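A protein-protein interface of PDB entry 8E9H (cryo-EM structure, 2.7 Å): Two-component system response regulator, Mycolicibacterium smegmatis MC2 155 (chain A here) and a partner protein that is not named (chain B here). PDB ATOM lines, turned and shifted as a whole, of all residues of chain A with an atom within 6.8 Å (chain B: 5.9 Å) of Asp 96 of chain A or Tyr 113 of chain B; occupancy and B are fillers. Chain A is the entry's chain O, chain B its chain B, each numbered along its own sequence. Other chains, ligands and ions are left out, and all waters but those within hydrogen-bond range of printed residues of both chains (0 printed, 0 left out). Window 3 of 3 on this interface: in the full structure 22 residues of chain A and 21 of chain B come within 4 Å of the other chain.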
ATOM      1  N   GLY A  93     -16.945   8.421 -20.340  1.00  0.00           N
ATOM      2  CA  GLY A  93     -17.285   9.822 -20.493  1.00  0.00           C
ATOM      3  C   GLY A  93     -17.430  10.286 -21.926  1.00  0.00           C
ATOM      4  O   GLY A  93     -17.858  11.424 -22.145  1.00  0.00           O
ATOM      5  N   ARG A  94     -17.084   9.452 -22.901  1.00  0.00           N
ATOM      6  CA  ARG A  94     -17.212   9.843 -24.296  1.00  0.00           C
ATOM      7  C   ARG A  94     -17.217   8.598 -25.166  1.00  0.00           C
ATOM      8  O   ARG A  94     -16.826   7.513 -24.733  1.00  0.00           O
ATOM      9  CB  ARG A  94     -16.086  10.783 -24.722  1.00  0.00           C
ATOM     10  CG  ARG A  94     -14.717  10.330 -24.280  1.00  0.00           C
ATOM     11  CD  ARG A  94     -13.635  11.039 -25.058  1.00  0.00           C
ATOM     12  NE  ARG A  94     -12.307  10.667 -24.595  1.00  0.00           N
ATOM     13  CZ  ARG A  94     -11.182  11.014 -25.201  1.00  0.00           C
ATOM     14  NH1 ARG A  94     -11.186  11.758 -26.293  1.00  0.00           N
ATOM     15  NH2 ARG A  94     -10.024  10.601 -24.701  1.00  0.00           N
ATOM     16  N   ALA A  95     -17.665   8.775 -26.409  1.00  0.00           N
ATOM     17  CA  ALA A  95     -17.721   7.654 -27.336  1.00  0.00           C
ATOM     18  C   ALA A  95     -16.332   7.104 -27.617  1.00  0.00           C
ATOM     19  O   ALA A  95     -16.133   5.885 -27.650  1.00  0.00           O
ATOM     20  CB  ALA A  95     -18.396   8.082 -28.637  1.00  0.00           C
ATOM     21  N   ASP A  96     -15.356   7.984 -27.817  1.00  0.00           N
ATOM     22  CA  ASP A  96     -14.013   7.535 -28.154  1.00  0.00           C
ATOM     23  C   ASP A  96     -13.339   6.783 -27.020  1.00  0.00           C
ATOM     24  O   ASP A  96     -12.316   6.135 -27.260  1.00  0.00           O
ATOM     25  CB  ASP A  96     -13.157   8.727 -28.569  1.00  0.00           C
ATOM     26  CG  ASP A  96     -13.719   9.446 -29.772  1.00  0.00           C
ATOM     27  OD1 ASP A  96     -14.651  10.258 -29.599  1.00  0.00           O
ATOM     28  OD2 ASP A  96     -13.237   9.193 -30.895  1.00  0.00           O
ATOM     29  N   ASP A  97     -13.870   6.846 -25.804  1.00  0.00           N
ATOM     30  CA  ASP A  97     -13.364   6.024 -24.717  1.00  0.00           C
ATOM     31  C   ASP A  97     -13.701   4.554 -24.896  1.00  0.00           C
ATOM     32  O   ASP A  97     -13.129   3.713 -24.195  1.00  0.00           O
ATOM     33  CB  ASP A  97     -13.925   6.510 -23.378  1.00  0.00           C
ATOM     34  CG  ASP A  97     -13.051   7.561 -22.723  1.00  0.00           C
ATOM     35  OD1 ASP A  97     -11.848   7.638 -23.052  1.00  0.00           O
ATOM     36  OD2 ASP A  97     -13.567   8.315 -21.872  1.00  0.00           O
ATOM     37  N   ALA A  98     -14.596   4.225 -25.830  1.00  0.00           N
ATOM     38  CA  ALA A  98     -15.000   2.838 -26.014  1.00  0.00           C
ATOM     39  C   ALA A  98     -13.800   1.922 -26.161  1.00  0.00           C
ATOM     40  O   ALA A  98     -13.761   0.846 -25.558  1.00  0.00           O
ATOM     41  CB  ALA A  98     -15.905   2.718 -27.239  1.00  0.00           C
ATOM     42  N   TRP A  99     -12.802   2.335 -26.941  1.00  0.00           N
ATOM     43  CA  TRP A  99     -11.615   1.508 -27.102  1.00  0.00           C
ATOM     44  C   TRP A  99     -11.005   1.160 -25.753  1.00  0.00           C
ATOM     45  O   TRP A  99     -10.790  -0.017 -25.449  1.00  0.00           O
ATOM     46  CB  TRP A  99     -10.598   2.224 -27.981  1.00  0.00           C
ATOM     47  CG  TRP A  99      -9.464   1.361 -28.396  1.00  0.00           C
ATOM     48  CD1 TRP A  99      -9.455   0.461 -29.415  1.00  0.00           C
ATOM     49  CD2 TRP A  99      -8.165   1.317 -27.808  1.00  0.00           C
ATOM     50  NE1 TRP A  99      -8.229  -0.146 -29.496  1.00  0.00           N
ATOM     51  CE2 TRP A  99      -7.418   0.366 -28.519  1.00  0.00           C
ATOM     52  CE3 TRP A  99      -7.559   1.991 -26.747  1.00  0.00           C
ATOM     53  CZ2 TRP A  99      -6.098   0.069 -28.206  1.00  0.00           C
ATOM     54  CZ3 TRP A  99      -6.251   1.696 -26.438  1.00  0.00           C
ATOM     55  CH2 TRP A  99      -5.534   0.745 -27.163  1.00  0.00           C
ATOM     56  N   LEU A 100     -10.755   2.164 -24.911  1.00  0.00           N
ATOM     57  CA  LEU A 100     -10.216   1.864 -23.592  1.00  0.00           C
ATOM     58  C   LEU A 100     -11.173   1.006 -22.787  1.00  0.00           C
ATOM     59  O   LEU A 100     -10.731   0.157 -22.007  1.00  0.00           O
ATOM     60  CB  LEU A 100      -9.904   3.146 -22.830  1.00  0.00           C
ATOM     61  CG  LEU A 100      -8.619   3.876 -23.204  1.00  0.00           C
ATOM     62  CD1 LEU A 100      -8.459   5.106 -22.340  1.00  0.00           C
ATOM     63  CD2 LEU A 100      -7.423   2.967 -23.049  1.00  0.00           C
ATOM     64  N   ALA A 101     -12.480   1.203 -22.957  1.00  0.00           N
ATOM     65  CA  ALA A 101     -13.430   0.342 -22.265  1.00  0.00           C
ATOM     66  C   ALA A 101     -13.177  -1.114 -22.614  1.00  0.00           C
ATOM     67  O   ALA A 101     -13.277  -1.993 -21.752  1.00  0.00           O
ATOM     68  CB  ALA A 101     -14.860   0.741 -22.617  1.00  0.00           C
ATOM     69  N   GLN B  78      -4.228   7.357 -26.880  1.00  0.00           N
ATOM     70  CA  GLN B  78      -5.080   6.196 -26.654  1.00  0.00           C
ATOM     71  C   GLN B  78      -4.274   4.909 -26.740  1.00  0.00           C
ATOM     72  O   GLN B  78      -4.366   4.043 -25.866  1.00  0.00           O
ATOM     73  CB  GLN B  78      -6.222   6.180 -27.667  1.00  0.00           C
ATOM     74  CG  GLN B  78      -7.208   7.316 -27.504  1.00  0.00           C
ATOM     75  CD  GLN B  78      -8.235   7.042 -26.435  1.00  0.00           C
ATOM     76  OE1 GLN B  78      -8.114   6.087 -25.675  1.00  0.00           O
ATOM     77  NE2 GLN B  78      -9.258   7.881 -26.370  1.00  0.00           N
ATOM     78  N   ASN B 111      -7.943  18.264 -26.334  1.00  0.00           N
ATOM     79  CA  ASN B 111      -9.246  17.711 -25.981  1.00  0.00           C
ATOM     80  C   ASN B 111      -9.874  17.093 -27.230  1.00  0.00           C
ATOM     81  O   ASN B 111     -10.727  17.676 -27.898  1.00  0.00           O
ATOM     82  CB  ASN B 111     -10.122  18.800 -25.386  1.00  0.00           C
ATOM     83  CG  ASN B 111     -11.409  18.267 -24.828  1.00  0.00           C
ATOM     84  OD1 ASN B 111     -11.645  17.062 -24.823  1.00  0.00           O
ATOM     85  ND2 ASN B 111     -12.255  19.163 -24.345  1.00  0.00           N
ATOM     86  N   ASN B 112      -9.427  15.880 -27.544  1.00  0.00           N
ATOM     87  CA  ASN B 112      -9.870  15.209 -28.756  1.00  0.00           C
ATOM     88  C   ASN B 112      -9.792  13.701 -28.565  1.00  0.00           C
ATOM     89  O   ASN B 112      -9.476  13.201 -27.485  1.00  0.00           O
ATOM     90  CB  ASN B 112      -9.035  15.645 -29.961  1.00  0.00           C
ATOM     91  CG  ASN B 112      -7.575  15.313 -29.804  1.00  0.00           C
ATOM     92  OD1 ASN B 112      -7.196  14.520 -28.949  1.00  0.00           O
ATOM     93  ND2 ASN B 112      -6.741  15.927 -30.625  1.00  0.00           N
ATOM     94  N   TYR B 113     -10.078  12.982 -29.651  1.00  0.00           N
ATOM     95  CA  TYR B 113     -10.163  11.527 -29.600  1.00  0.00           C
ATOM     96  C   TYR B 113      -8.850  10.890 -29.168  1.00  0.00           C
ATOM     97  O   TYR B 113      -8.840   9.938 -28.381  1.00  0.00           O
ATOM     98  CB  TYR B 113     -10.565  10.993 -30.974  1.00  0.00           C
ATOM     99  CG  TYR B 113      -9.530  11.281 -32.030  1.00  0.00           C
ATOM    100  CD1 TYR B 113      -9.449  12.526 -32.628  1.00  0.00           C
ATOM    101  CD2 TYR B 113      -8.612  10.320 -32.408  1.00  0.00           C
ATOM    102  CE1 TYR B 113      -8.498  12.799 -33.577  1.00  0.00           C
ATOM    103  CE2 TYR B 113      -7.657  10.585 -33.357  1.00  0.00           C
ATOM    104  CZ  TYR B 113      -7.600  11.828 -33.933  1.00  0.00           C
ATOM    105  OH  TYR B 113      -6.649  12.093 -34.885  1.00  0.00           O
ATOM    106  N   ALA B 114      -7.727  11.392 -29.681  1.00  0.00           N
ATOM    107  CA  ALA B 114      -6.473  10.656 -29.598  1.00  0.00           C
ATOM    108  C   ALA B 114      -5.878  10.640 -28.200  1.00  0.00           C
ATOM    109  O   ALA B 114      -5.107   9.730 -27.887  1.00  0.00           O
ATOM    110  CB  ALA B 114      -5.456  11.251 -30.567  1.00  0.00           C
ATOM    111  N   VAL B 115      -6.200  11.616 -27.360  1.00  0.00           N
ATOM    112  CA  VAL B 115      -5.582  11.753 -26.049  1.00  0.00           C
ATOM    113  C   VAL B 115      -6.551  11.237 -24.998  1.00  0.00           C
ATOM    114  O   VAL B 115      -7.770  11.308 -25.177  1.00  0.00           O
ATOM    115  CB  VAL B 115      -5.185  13.212 -25.761  1.00  0.00           C
ATOM    116  CG1 VAL B 115      -4.463  13.311 -24.437  1.00  0.00           C
ATOM    117  CG2 VAL B 115      -4.319  13.744 -26.874  1.00  0.00           C
ATOM    118  N   VAL B 116      -6.001  10.719 -23.896  1.00  0.00           N
ATOM    119  CA  VAL B 116      -6.806  10.048 -22.878  1.00  0.00           C
ATOM    120  C   VAL B 116      -7.543  11.013 -21.967  1.00  0.00           C
ATOM    121  O   VAL B 116      -8.422  10.582 -21.212  1.00  0.00           O
ATOM    122  CB  VAL B 116      -5.905   9.115 -22.045  1.00  0.00           C
ATOM    123  CG1 VAL B 116      -6.663   8.529 -20.875  1.00  0.00           C
ATOM    124  CG2 VAL B 116      -5.361   8.008 -22.915  1.00  0.00           C
ATOM    125  N   GLN B 117      -7.232  12.304 -22.023  1.00  0.00           N
ATOM    126  CA  GLN B 117      -7.887  13.297 -21.173  1.00  0.00           C
ATOM    127  C   GLN B 117      -7.582  13.043 -19.703  1.00  0.00           C
ATOM    128  O   GLN B 117      -8.482  12.949 -18.869  1.00  0.00           O
ATOM    129  CB  GLN B 117      -9.397  13.325 -21.413  1.00  0.00           C
ATOM    130  CG  GLN B 117      -9.784  13.629 -22.840  1.00  0.00           C
ATOM    131  CD  GLN B 117      -9.057  14.834 -23.384  1.00  0.00           C
ATOM    132  OE1 GLN B 117      -9.111  15.915 -22.806  1.00  0.00           O
ATOM    133  NE2 GLN B 117      -8.360  14.650 -24.494  1.00  0.00           N
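Of chain B, only Gln 78 (3.6 Å) and Tyr 113 (3.2 Å) come within 4 Å of Asp 96 of chain A.
Printed residues of chain B within 4 Å of Leu 100 of chain A: Gln 78.
Printed residues of chain A within 4 Å of Gln 78 of chain B: Arg 94 (3.3 Å), Asp 96 (3.6 Å), Trp 99 (3.1 Å) and Leu 100 (3.4 Å).
Tyr 113 of chain B touches just these residues of chain A: Arg 94 (3.5 Å) and Asp 96 (3.2 Å).
Of the printed residues of chain A, Val 116 of chain B touches Arg 94.
The nearest residue of chain A that does not touch Tyr 113 of chain B is Asp 97 of chain A (6.4 Å).
The backbone carbonyl oxygen (O) of Tyr 113 of chain B sits at hydrogen-bond distance from the side-chain amide nitrogen (NE2) of Gln 78 of chain B (2.9 Å).
The backbone NH of Gln 78 of chain B lies within hydrogen-bond range of the backbone carbonyl oxygen of Ala 114 of chain B, 2.7 Å away.
The side-chain amide oxygen (OD1) of Asn 111 of chain B sits close to the side-chain amide oxygen (OE1) of Gln 117 of chain B (3.4 Å).
OD1 of Asn 112 of chain B lies within hydrogen-bond range of N of Ala 114 of chain B (3.3 Å).
The side-chain amide oxygen of Asn 112 of chain B is in hydrogen-bond range of the backbone NH of Val 115 of chain B.
NE2 of Gln 117 of chain B lies close to N of Asn 112 of chain B (3.5 Å).
Arg 94 of chain A touches Tyr 113 of chain B.
Arg 94 of chain A touches Val 116 of chain B (NH2 to C, 3.7 Å).
NH2 of Arg 94 of chain A touches CG of Gln 117 of chain B, 3.6 Å away.
Gln 78 of chain B touches Asp 96 of chain A.
Asp 96 of chain A touches Tyr 113 of chain B.
Gln 78 of chain B touches Trp 99 of chain A (O to CZ3, 3.1 Å).
Leu 100 of chain A touches Gln 78 of chain B.
NE2 of Gln 78 of chain B sits close to NH2 of Arg 94 of chain A (3.3 Å).
The backbone carbonyl oxygen (O) of Asn 112 of chain B sits at hydrogen-bond distance from the guanidinium group (NH1) of Arg 94 of chain A, 2.5 Å away.
The guanidinium group (NH2) of Arg 94 of chain A is in hydrogen-bond range of the backbone carbonyl oxygen (O) of Val 115 of chain B (2.4 Å).
Of the 9 printed residues of chain A, 4 touch a printed residue of chain B.
Hydrophobic or aromatic side chains of chain A within 4 Å of the printed part of chain B: Trp 99 and Leu 100.
Along chain A the printed residues that touch a printed residue of chain B span positions 94 to 100.
Printed residues of chain B that touch a printed residue of chain A: Gln 78, Asn 112, Tyr 113, Val 115, Val 116 and Gln 117.
Hydrophobic or aromatic side chains of chain B within 4 Å of the printed part of chain A: Tyr 113.
Among the printed residues, no Asp or Glu carboxylate lies within 4 Å of a Lys or Arg side-chain nitrogen of the other chain.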
